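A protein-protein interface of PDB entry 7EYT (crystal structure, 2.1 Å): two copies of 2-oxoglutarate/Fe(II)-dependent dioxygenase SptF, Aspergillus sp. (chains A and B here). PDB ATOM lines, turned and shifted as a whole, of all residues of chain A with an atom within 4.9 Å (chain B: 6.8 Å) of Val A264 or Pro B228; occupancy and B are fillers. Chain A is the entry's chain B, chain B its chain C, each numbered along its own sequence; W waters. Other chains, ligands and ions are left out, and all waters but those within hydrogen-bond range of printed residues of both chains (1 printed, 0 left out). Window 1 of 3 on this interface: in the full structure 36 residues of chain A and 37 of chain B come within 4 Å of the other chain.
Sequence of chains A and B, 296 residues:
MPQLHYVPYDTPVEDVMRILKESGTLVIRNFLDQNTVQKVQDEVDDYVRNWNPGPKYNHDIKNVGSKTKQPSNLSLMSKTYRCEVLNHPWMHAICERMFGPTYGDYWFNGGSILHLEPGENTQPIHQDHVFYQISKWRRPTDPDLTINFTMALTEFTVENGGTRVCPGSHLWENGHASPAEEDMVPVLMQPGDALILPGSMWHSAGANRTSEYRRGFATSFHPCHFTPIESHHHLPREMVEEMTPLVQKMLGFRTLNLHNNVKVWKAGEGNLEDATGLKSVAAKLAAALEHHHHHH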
ATOM      1  N   CYS A 224     -25.139  22.165   7.105  1.00  0.00           N
ATOM      2  CA  CYS A 224     -25.113  21.939   5.664  1.00  0.00           C
ATOM      3  C   CYS A 224     -25.247  20.467   5.295  1.00  0.00           C
ATOM      4  O   CYS A 224     -25.668  20.161   4.174  1.00  0.00           O
ATOM      5  CB  CYS A 224     -23.823  22.508   5.068  1.00  0.00           C
ATOM      6  SG  CYS A 224     -22.310  21.627   5.541  1.00  0.00           S
ATOM      7  N   HIS A 225     -24.907  19.553   6.200  1.00  0.00           N
ATOM      8  CA  HIS A 225     -25.005  18.130   5.901  1.00  0.00           C
ATOM      9  C   HIS A 225     -26.422  17.587   6.042  1.00  0.00           C
ATOM     10  O   HIS A 225     -26.628  16.388   5.822  1.00  0.00           O
ATOM     11  CB  HIS A 225     -24.054  17.331   6.800  1.00  0.00           C
ATOM     12  CG  HIS A 225     -23.379  16.192   6.100  1.00  0.00           C
ATOM     13  ND1 HIS A 225     -22.219  15.614   6.568  1.00  0.00           N
ATOM     14  CD2 HIS A 225     -23.700  15.526   4.967  1.00  0.00           C
ATOM     15  CE1 HIS A 225     -21.854  14.640   5.752  1.00  0.00           C
ATOM     16  NE2 HIS A 225     -22.737  14.567   4.772  1.00  0.00           N
ATOM     17  N   THR A 255     -21.655  25.015  -3.405  1.00  0.00           N
ATOM     18  CA  THR A 255     -21.061  23.902  -2.678  1.00  0.00           C
ATOM     19  C   THR A 255     -20.825  24.290  -1.222  1.00  0.00           C
ATOM     20  O   THR A 255     -20.465  25.431  -0.918  1.00  0.00           O
ATOM     21  CB  THR A 255     -19.748  23.488  -3.349  1.00  0.00           C
ATOM     22  OG1 THR A 255     -20.036  22.922  -4.632  1.00  0.00           O
ATOM     23  CG2 THR A 255     -18.994  22.464  -2.513  1.00  0.00           C
ATOM     24  N   LEU A 256     -21.051  23.342  -0.320  1.00  0.00           N
ATOM     25  CA  LEU A 256     -20.933  23.573   1.111  1.00  0.00           C
ATOM     26  C   LEU A 256     -19.691  22.884   1.659  1.00  0.00           C
ATOM     27  O   LEU A 256     -19.281  21.825   1.174  1.00  0.00           O
ATOM     28  CB  LEU A 256     -22.176  23.069   1.846  1.00  0.00           C
ATOM     29  CG  LEU A 256     -23.503  23.602   1.304  1.00  0.00           C
ATOM     30  CD1 LEU A 256     -24.552  22.503   1.298  1.00  0.00           C
ATOM     31  CD2 LEU A 256     -23.976  24.803   2.109  1.00  0.00           C
ATOM     32  N   LEU A 258     -17.812  21.187   4.915  1.00  0.00           N
ATOM     33  CA  LEU A 258     -18.011  20.571   6.215  1.00  0.00           C
ATOM     34  C   LEU A 258     -16.951  21.056   7.202  1.00  0.00           C
ATOM     35  O   LEU A 258     -16.026  21.796   6.857  1.00  0.00           O
ATOM     36  CB  LEU A 258     -17.974  19.048   6.101  1.00  0.00           C
ATOM     37  CG  LEU A 258     -19.102  18.389   5.306  1.00  0.00           C
ATOM     38  CD1 LEU A 258     -18.850  16.898   5.153  1.00  0.00           C
ATOM     39  CD2 LEU A 258     -20.446  18.641   5.973  1.00  0.00           C
ATOM     40  N   VAL A 262     -14.111  18.565   3.987  1.00  0.00           N
ATOM     41  CA  VAL A 262     -14.719  17.809   2.901  1.00  0.00           C
ATOM     42  C   VAL A 262     -15.933  18.573   2.391  1.00  0.00           C
ATOM     43  O   VAL A 262     -16.736  19.094   3.177  1.00  0.00           O
ATOM     44  CB  VAL A 262     -15.103  16.397   3.376  1.00  0.00           C
ATOM     45  CG1 VAL A 262     -15.978  15.696   2.343  1.00  0.00           C
ATOM     46  CG2 VAL A 262     -13.855  15.577   3.670  1.00  0.00           C
ATOM     47  N   LYS A 263     -16.064  18.667   1.072  1.00  0.00           N
ATOM     48  CA  LYS A 263     -17.154  19.418   0.470  1.00  0.00           C
ATOM     49  C   LYS A 263     -18.329  18.503   0.148  1.00  0.00           C
ATOM     50  O   LYS A 263     -18.147  17.379  -0.325  1.00  0.00           O
ATOM     51  CB  LYS A 263     -16.686  20.127  -0.802  1.00  0.00           C
ATOM     52  CG  LYS A 263     -15.679  21.238  -0.572  1.00  0.00           C
ATOM     53  CD  LYS A 263     -15.106  21.732  -1.893  1.00  0.00           C
ATOM     54  CE  LYS A 263     -14.266  22.985  -1.706  1.00  0.00           C
ATOM     55  NZ  LYS A 263     -15.105  24.192  -1.475  1.00  0.00           N
ATOM     56  N   VAL A 264     -19.534  18.992   0.417  1.00  0.00           N
ATOM     57  CA  VAL A 264     -20.759  18.333  -0.008  1.00  0.00           C
ATOM     58  C   VAL A 264     -21.450  19.232  -1.028  1.00  0.00           C
ATOM     59  O   VAL A 264     -21.109  20.405  -1.188  1.00  0.00           O
ATOM     60  CB  VAL A 264     -21.692  18.012   1.176  1.00  0.00           C
ATOM     61  CG1 VAL A 264     -21.026  17.036   2.130  1.00  0.00           C
ATOM     62  CG2 VAL A 264     -22.100  19.293   1.899  1.00  0.00           C
ATOM     63  N   TRP A 265     -22.435  18.663  -1.728  1.00  0.00           N
ATOM     64  CA  TRP A 265     -23.223  19.406  -2.714  1.00  0.00           C
ATOM     65  C   TRP A 265     -22.333  19.940  -3.836  1.00  0.00           C
ATOM     66  O   TRP A 265     -22.510  21.061  -4.317  1.00  0.00           O
ATOM     67  CB  TRP A 265     -24.011  20.539  -2.045  1.00  0.00           C
ATOM     68  CG  TRP A 265     -25.253  20.966  -2.775  1.00  0.00           C
ATOM     69  CD1 TRP A 265     -25.557  22.227  -3.196  1.00  0.00           C
ATOM     70  CD2 TRP A 265     -26.362  20.139  -3.153  1.00  0.00           C
ATOM     71  NE1 TRP A 265     -26.782  22.238  -3.817  1.00  0.00           N
ATOM     72  CE2 TRP A 265     -27.297  20.968  -3.805  1.00  0.00           C
ATOM     73  CE3 TRP A 265     -26.653  18.779  -3.009  1.00  0.00           C
ATOM     74  CZ2 TRP A 265     -28.501  20.483  -4.311  1.00  0.00           C
ATOM     75  CZ3 TRP A 265     -27.850  18.299  -3.512  1.00  0.00           C
ATOM     76  CH2 TRP A 265     -28.758  19.148  -4.156  1.00  0.00           C
ATOM     77  N   LYS A 266     -21.366  19.129  -4.251  1.00  0.00           N
ATOM     78  CA  LYS A 266     -20.435  19.499  -5.303  1.00  0.00           C
ATOM     79  C   LYS A 266     -20.987  19.127  -6.675  1.00  0.00           C
ATOM     80  O   LYS A 266     -21.914  18.324  -6.806  1.00  0.00           O
ATOM     81  CB  LYS A 266     -19.084  18.812  -5.099  1.00  0.00           C
ATOM     82  CG  LYS A 266     -18.612  18.732  -3.663  1.00  0.00           C
ATOM     83  CD  LYS A 266     -17.295  17.973  -3.575  1.00  0.00           C
ATOM     84  CE  LYS A 266     -17.469  16.515  -3.969  1.00  0.00           C
ATOM     85  NZ  LYS A 266     -16.172  15.786  -4.001  1.00  0.00           N
ATOM     86  N   TYR B  57      -9.284  18.824  -4.341  1.00  0.00           N
ATOM     87  CA  TYR B  57      -9.218  19.893  -3.356  1.00  0.00           C
ATOM     88  C   TYR B  57      -8.665  19.333  -2.052  1.00  0.00           C
ATOM     89  O   TYR B  57      -8.519  18.121  -1.880  1.00  0.00           O
ATOM     90  CB  TYR B  57     -10.590  20.545  -3.134  1.00  0.00           C
ATOM     91  CG  TYR B  57     -11.646  19.609  -2.587  1.00  0.00           C
ATOM     92  CD1 TYR B  57     -12.370  18.776  -3.430  1.00  0.00           C
ATOM     93  CD2 TYR B  57     -11.926  19.567  -1.227  1.00  0.00           C
ATOM     94  CE1 TYR B  57     -13.339  17.922  -2.934  1.00  0.00           C
ATOM     95  CE2 TYR B  57     -12.893  18.717  -0.721  1.00  0.00           C
ATOM     96  CZ  TYR B  57     -13.595  17.898  -1.578  1.00  0.00           C
ATOM     97  OH  TYR B  57     -14.557  17.050  -1.077  1.00  0.00           O
ATOM     98  N   TRP B 107     -31.648   8.705  -1.315  1.00  0.00           N
ATOM     99  CA  TRP B 107     -31.255   9.208  -2.624  1.00  0.00           C
ATOM    100  C   TRP B 107     -29.749   9.057  -2.796  1.00  0.00           C
ATOM    101  O   TRP B 107     -29.037   8.602  -1.895  1.00  0.00           O
ATOM    102  CB  TRP B 107     -31.708  10.661  -2.835  1.00  0.00           C
ATOM    103  CG  TRP B 107     -31.262  11.666  -1.798  1.00  0.00           C
ATOM    104  CD1 TRP B 107     -30.670  11.413  -0.594  1.00  0.00           C
ATOM    105  CD2 TRP B 107     -31.390  13.092  -1.888  1.00  0.00           C
ATOM    106  NE1 TRP B 107     -30.421  12.593   0.069  1.00  0.00           N
ATOM    107  CE2 TRP B 107     -30.853  13.638  -0.705  1.00  0.00           C
ATOM    108  CE3 TRP B 107     -31.905  13.960  -2.857  1.00  0.00           C
ATOM    109  CZ2 TRP B 107     -30.819  15.011  -0.464  1.00  0.00           C
ATOM    110  CZ3 TRP B 107     -31.869  15.322  -2.619  1.00  0.00           C
ATOM    111  CH2 TRP B 107     -31.328  15.834  -1.432  1.00  0.00           C
ATOM    112  N   PHE B 108     -29.275   9.438  -3.980  1.00  0.00           N
ATOM    113  CA  PHE B 108     -27.872   9.287  -4.339  1.00  0.00           C
ATOM    114  C   PHE B 108     -27.000  10.167  -3.454  1.00  0.00           C
ATOM    115  O   PHE B 108     -27.291  11.351  -3.255  1.00  0.00           O
ATOM    116  CB  PHE B 108     -27.677   9.648  -5.812  1.00  0.00           C
ATOM    117  CG  PHE B 108     -26.356   9.217  -6.385  1.00  0.00           C
ATOM    118  CD1 PHE B 108     -26.046   7.875  -6.517  1.00  0.00           C
ATOM    119  CD2 PHE B 108     -25.434  10.158  -6.812  1.00  0.00           C
ATOM    120  CE1 PHE B 108     -24.835   7.479  -7.054  1.00  0.00           C
ATOM    121  CE2 PHE B 108     -24.221   9.769  -7.349  1.00  0.00           C
ATOM    122  CZ  PHE B 108     -23.923   8.428  -7.471  1.00  0.00           C
ATOM    123  N   ASN B 109     -25.936   9.583  -2.906  1.00  0.00           N
ATOM    124  CA  ASN B 109     -24.954  10.351  -2.149  1.00  0.00           C
ATOM    125  C   ASN B 109     -23.820  10.813  -3.059  1.00  0.00           C
ATOM    126  O   ASN B 109     -23.606  12.015  -3.238  1.00  0.00           O
ATOM    127  CB  ASN B 109     -24.413   9.514  -0.984  1.00  0.00           C
ATOM    128  CG  ASN B 109     -23.604  10.337   0.003  1.00  0.00           C
ATOM    129  OD1 ASN B 109     -23.496  11.557  -0.125  1.00  0.00           O
ATOM    130  ND2 ASN B 109     -23.033   9.672   0.996  1.00  0.00           N
ATOM    131  N   GLY B 110     -23.099   9.864  -3.646  1.00  0.00           N
ATOM    132  CA  GLY B 110     -22.022  10.169  -4.569  1.00  0.00           C
ATOM    133  C   GLY B 110     -21.569   8.905  -5.263  1.00  0.00           C
ATOM    134  O   GLY B 110     -21.958   7.792  -4.894  1.00  0.00           O
ATOM    135  N   PHE B 131     -16.798  11.040   7.246  1.00  0.00           N
ATOM    136  CA  PHE B 131     -17.027  12.451   6.964  1.00  0.00           C
ATOM    137  C   PHE B 131     -18.390  12.939   7.442  1.00  0.00           C
ATOM    138  O   PHE B 131     -18.739  14.096   7.188  1.00  0.00           O
ATOM    139  CB  PHE B 131     -16.852  12.734   5.467  1.00  0.00           C
ATOM    140  CG  PHE B 131     -17.940  12.167   4.596  1.00  0.00           C
ATOM    141  CD1 PHE B 131     -17.934  10.831   4.236  1.00  0.00           C
ATOM    142  CD2 PHE B 131     -18.953  12.982   4.114  1.00  0.00           C
ATOM    143  CE1 PHE B 131     -18.929  10.311   3.425  1.00  0.00           C
ATOM    144  CE2 PHE B 131     -19.950  12.470   3.303  1.00  0.00           C
ATOM    145  CZ  PHE B 131     -19.936  11.133   2.957  1.00  0.00           C
ATOM    146  N   TYR B 132     -19.159  12.095   8.129  1.00  0.00           N
ATOM    147  CA  TYR B 132     -20.382  12.521   8.798  1.00  0.00           C
ATOM    148  C   TYR B 132     -20.049  12.886  10.239  1.00  0.00           C
ATOM    149  O   TYR B 132     -19.511  12.059  10.982  1.00  0.00           O
ATOM    150  CB  TYR B 132     -21.443  11.422   8.775  1.00  0.00           C
ATOM    151  CG  TYR B 132     -22.032  11.125   7.418  1.00  0.00           C
ATOM    152  CD1 TYR B 132     -21.428  10.214   6.565  1.00  0.00           C
ATOM    153  CD2 TYR B 132     -23.203  11.743   6.996  1.00  0.00           C
ATOM    154  CE1 TYR B 132     -21.966   9.932   5.328  1.00  0.00           C
ATOM    155  CE2 TYR B 132     -23.749  11.468   5.756  1.00  0.00           C
ATOM    156  CZ  TYR B 132     -23.125  10.560   4.926  1.00  0.00           C
ATOM    157  OH  TYR B 132     -23.658  10.277   3.689  1.00  0.00           O
ATOM    158  N   HIS B 222     -27.752   7.214   0.491  1.00  0.00           N
ATOM    159  CA  HIS B 222     -27.858   7.527   1.910  1.00  0.00           C
ATOM    160  C   HIS B 222     -29.238   8.109   2.169  1.00  0.00           C
ATOM    161  O   HIS B 222     -29.973   8.431   1.226  1.00  0.00           O
ATOM    162  CB  HIS B 222     -26.739   8.485   2.351  1.00  0.00           C
ATOM    163  CG  HIS B 222     -26.867   9.879   1.819  1.00  0.00           C
ATOM    164  ND1 HIS B 222     -26.179  10.942   2.364  1.00  0.00           N
ATOM    165  CD2 HIS B 222     -27.586  10.386   0.790  1.00  0.00           C
ATOM    166  CE1 HIS B 222     -26.475  12.043   1.699  1.00  0.00           C
ATOM    167  NE2 HIS B 222     -27.329  11.735   0.740  1.00  0.00           N
ATOM    168  N   PRO B 223     -29.642   8.217   3.441  1.00  0.00           N
ATOM    169  CA  PRO B 223     -30.979   8.739   3.756  1.00  0.00           C
ATOM    170  C   PRO B 223     -31.262  10.085   3.102  1.00  0.00           C
ATOM    171  O   PRO B 223     -30.355  10.869   2.817  1.00  0.00           O
ATOM    172  CB  PRO B 223     -30.953   8.861   5.282  1.00  0.00           C
ATOM    173  CG  PRO B 223     -30.037   7.784   5.713  1.00  0.00           C
ATOM    174  CD  PRO B 223     -29.003   7.623   4.631  1.00  0.00           C
ATOM    175  N   CYS B 224     -32.553  10.349   2.878  1.00  0.00           N
ATOM    176  CA  CYS B 224     -32.961  11.565   2.187  1.00  0.00           C
ATOM    177  C   CYS B 224     -32.764  12.815   3.034  1.00  0.00           C
ATOM    178  O   CYS B 224     -32.694  13.915   2.478  1.00  0.00           O
ATOM    179  CB  CYS B 224     -34.423  11.457   1.750  1.00  0.00           C
ATOM    180  SG  CYS B 224     -35.612  11.337   3.105  1.00  0.00           S
ATOM    181  N   PHE B 226     -30.103  13.575   4.556  1.00  0.00           N
ATOM    182  CA  PHE B 226     -28.680  13.884   4.540  1.00  0.00           C
ATOM    183  C   PHE B 226     -28.308  14.509   3.201  1.00  0.00           C
ATOM    184  O   PHE B 226     -28.772  14.063   2.146  1.00  0.00           O
ATOM    185  CB  PHE B 226     -27.832  12.629   4.778  1.00  0.00           C
ATOM    186  CG  PHE B 226     -28.079  11.960   6.104  1.00  0.00           C
ATOM    187  CD1 PHE B 226     -28.706  12.637   7.139  1.00  0.00           C
ATOM    188  CD2 PHE B 226     -27.679  10.650   6.313  1.00  0.00           C
ATOM    189  CE1 PHE B 226     -28.933  12.018   8.355  1.00  0.00           C
ATOM    190  CE2 PHE B 226     -27.901  10.026   7.528  1.00  0.00           C
ATOM    191  CZ  PHE B 226     -28.529  10.710   8.549  1.00  0.00           C
ATOM    192  N   THR B 227     -27.470  15.536   3.250  1.00  0.00           N
ATOM    193  CA  THR B 227     -27.068  16.237   2.034  1.00  0.00           C
ATOM    194  C   THR B 227     -26.066  15.393   1.253  1.00  0.00           C
ATOM    195  O   THR B 227     -25.052  14.969   1.817  1.00  0.00           O
ATOM    196  CB  THR B 227     -26.453  17.593   2.372  1.00  0.00           C
ATOM    197  OG1 THR B 227     -27.362  18.341   3.190  1.00  0.00           O
ATOM    198  CG2 THR B 227     -26.157  18.378   1.104  1.00  0.00           C
ATOM    199  N   PRO B 228     -26.306  15.139  -0.031  1.00  0.00           N
ATOM    200  CA  PRO B 228     -25.368  14.322  -0.807  1.00  0.00           C
ATOM    201  C   PRO B 228     -24.050  15.045  -1.023  1.00  0.00           C
ATOM    202  O   PRO B 228     -23.983  16.277  -1.044  1.00  0.00           O
ATOM    203  CB  PRO B 228     -26.098  14.099  -2.139  1.00  0.00           C
ATOM    204  CG  PRO B 228     -27.519  14.566  -1.910  1.00  0.00           C
ATOM    205  CD  PRO B 228     -27.435  15.607  -0.850  1.00  0.00           C
ATOM    206  N   ILE B 229     -22.986  14.256  -1.181  1.00  0.00           N
ATOM    207  CA  ILE B 229     -21.683  14.847  -1.464  1.00  0.00           C
ATOM    208  C   ILE B 229     -21.673  15.463  -2.857  1.00  0.00           C
ATOM    209  O   ILE B 229     -20.919  16.407  -3.123  1.00  0.00           O
ATOM    210  CB  ILE B 229     -20.567  13.798  -1.293  1.00  0.00           C
ATOM    211  CG1 ILE B 229     -19.196  14.473  -1.240  1.00  0.00           C
ATOM    212  CG2 ILE B 229     -20.599  12.782  -2.418  1.00  0.00           C
ATOM    213  CD1 ILE B 229     -18.311  13.972  -0.120  1.00  0.00           C
ATOM    214  N   GLU B 230     -22.523  14.967  -3.755  1.00  0.00           N
ATOM    215  CA  GLU B 230     -22.574  15.419  -5.138  1.00  0.00           C
ATOM    216  C   GLU B 230     -23.961  15.956  -5.455  1.00  0.00           C
ATOM    217  O   GLU B 230     -24.962  15.259  -5.254  1.00  0.00           O
ATOM    218  CB  GLU B 230     -22.230  14.280  -6.101  1.00  0.00           C
ATOM    219  CG  GLU B 230     -20.745  14.036  -6.286  1.00  0.00           C
ATOM    220  CD  GLU B 230     -20.472  12.915  -7.265  1.00  0.00           C
ATOM    221  OE1 GLU B 230     -20.548  13.161  -8.486  1.00  0.00           O
ATOM    222  OE2 GLU B 230     -20.194  11.785  -6.811  1.00  0.00           O
ATOM    223  N   SER B 231     -24.015  17.185  -5.953  1.00  0.00           N
ATOM    224  CA  SER B 231     -25.240  17.740  -6.504  1.00  0.00           C
ATOM    225  C   SER B 231     -25.361  17.360  -7.979  1.00  0.00           C
ATOM    226  O   SER B 231     -24.406  16.899  -8.609  1.00  0.00           O
ATOM    227  CB  SER B 231     -25.269  19.259  -6.331  1.00  0.00           C
ATOM    228  OG  SER B 231     -26.344  19.839  -7.049  1.00  0.00           O
ATOM    229  N   HIS B 232     -26.561  17.549  -8.531  1.00  0.00           N
ATOM    230  CA  HIS B 232     -26.778  17.250  -9.942  1.00  0.00           C
ATOM    231  C   HIS B 232     -27.618  18.320 -10.631  1.00  0.00           C
ATOM    232  O   HIS B 232     -28.149  18.073 -11.720  1.00  0.00           O
ATOM    233  CB  HIS B 232     -27.431  15.875 -10.116  1.00  0.00           C
ATOM    234  CG  HIS B 232     -26.541  14.736  -9.733  1.00  0.00           C
ATOM    235  ND1 HIS B 232     -26.524  14.201  -8.462  1.00  0.00           N
ATOM    236  CD2 HIS B 232     -25.629  14.038 -10.448  1.00  0.00           C
ATOM    237  CE1 HIS B 232     -25.643  13.218  -8.412  1.00  0.00           C
ATOM    238  NE2 HIS B 232     -25.085  13.099  -9.604  1.00  0.00           N
ATOM    239  N   MET B 250     -33.441   9.949  -7.127  1.00  0.00           N
ATOM    240  CA  MET B 250     -32.090   9.657  -6.656  1.00  0.00           C
ATOM    241  C   MET B 250     -31.183  10.873  -6.805  1.00  0.00           C
ATOM    242  O   MET B 250     -30.390  11.180  -5.908  1.00  0.00           O
ATOM    243  CB  MET B 250     -31.512   8.465  -7.423  1.00  0.00           C
ATOM    244  CG  MET B 250     -32.110   7.107  -7.061  1.00  0.00           C
ATOM    245  SD  MET B 250     -32.186   6.762  -5.294  1.00  0.00           S
ATOM    246  CE  MET B 250     -33.955   6.595  -5.062  1.00  0.00           C
ATOM    247  N   GLY B 252     -31.868  14.130  -6.984  1.00  0.00           N
ATOM    248  CA  GLY B 252     -32.228  15.388  -6.356  1.00  0.00           C
ATOM    249  C   GLY B 252     -33.215  16.258  -7.103  1.00  0.00           C
ATOM    250  O   GLY B 252     -33.239  17.472  -6.871  1.00  0.00           O
HETATM  251  O   HOH W   1     -22.859  13.287   2.138  1.00  0.00           O
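OH of Tyr B57 lies within hydrogen-bond range of N of Lys A263. The backbone carbonyl oxygen of Cys A224 lies within hydrogen-bond range of the side-chain hydroxyl of Thr B227. The backbone carbonyl oxygen (O) of His A225 is in hydrogen-bond range of the backbone NH (N) of Thr B227, 2.8 Å away. The backbone NH of Trp A265 sits at hydrogen-bond distance from the backbone carbonyl oxygen of Pro B228 (2.9 Å). The backbone carbonyl oxygen (O) of Ile B229 is in hydrogen-bond range of the backbone NH (N) of Trp A265 (3.1 Å). O of Ile B229 is in hydrogen-bond range of N of Lys A266 (3.0 Å). The backbone NH of Ser B231 lies within hydrogen-bond range of the backbone carbonyl oxygen of Lys A266 (2.5 Å).
The indole nitrogen of Trp B107 lies within hydrogen-bond range of the backbone carbonyl oxygen of Phe B226. OH of Tyr B132 is in hydrogen-bond range of ND2 of Asn B109. OD1 of Asn B109 lies within hydrogen-bond range of N of Ile B229 (2.9 Å). The backbone carbonyl oxygen (O) of Asn B109 sits at hydrogen-bond distance from the backbone NH (N) of Glu B230, at 3.2 Å. A ring nitrogen (NE2) of His B222 is in hydrogen-bond range of the backbone carbonyl oxygen (O) of Phe B226 (3.1 Å). N of Val A264 sits at hydrogen-bond distance from O of Leu A256 (2.9 Å).
Among the printed residues, merely in contact across the chains: Lys A263 with Ile B229 (3.2 Å), His A225 with Tyr B132 (3.4 Å), Lys A266 with Glu B230 (3.4 Å), Leu A258 with Phe B131 (3.5 Å), His A225 with Phe B131 (3.5 Å), Trp A265 with Ser B231 (3.5 Å), His A225 with Phe B226 (3.5 Å), Val A264 with Ile B229 (3.6 Å), Lys A266 with Tyr B57 (3.6 Å), Val A264 with Pro B228 (3.6 Å), Val A262 with Ile B229 (3.8 Å) and Val A262 with Tyr B57 (3.9 Å).
Of the printed residues of chain B, Lys A263 touches Tyr B57 (3.1 Å) and Ile B229 (3.2 Å). Val A264 touches two residues of chain B. Pro B223 touches none of the printed residues of chain A. Pro B228 touches two residues of chain A. Printed residues of chain A within 4 Å of Ser B231: Trp A265 and Lys A266. The nearest printed residue of chain A that does not touch Ile B229 is His A225 (6.0 Å).
Of the 10 printed residues of chain A, 8 touch a printed residue of chain B. Hydrophobic or aromatic side chains of chain A within 4 Å of the printed part of chain B: His A225, Leu A258, Val A262, Val A264 and Trp A265. Of the 19 printed residues of chain B, 9 touch a printed residue of chain A. Printed residues of chain B that touch a printed residue of chain A: Tyr B57, Phe B131, Tyr B132, Phe B226, Thr B227, Pro B228, Ile B229, Glu B230 and Ser B231. Hydrophobic or aromatic side chains of chain B within 4 Å of the printed part of chain A: Tyr B57, Phe B131, Tyr B132, Pro B228 and Ile B229. Among the printed residues, 19 pairs touch across the chains.
1 position is printed for both chains. Of the 19 pairs that touch across the chains among the printed residues, none has its exchanged pair printed and touching as well.
Water W1 lies within hydrogen-bond range of the backbone carbonyl oxygen (O) of Thr B227 (2.8 Å), the side-chain amide oxygen (OD1) of Asn B109 (2.9 Å), a ring nitrogen (NE2) of His A225 (2.9 Å), the backbone NH (N) of Ile B229 (3.5 Å) and the side-chain hydroxyl (OH) of Tyr B132 (3.5 Å).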
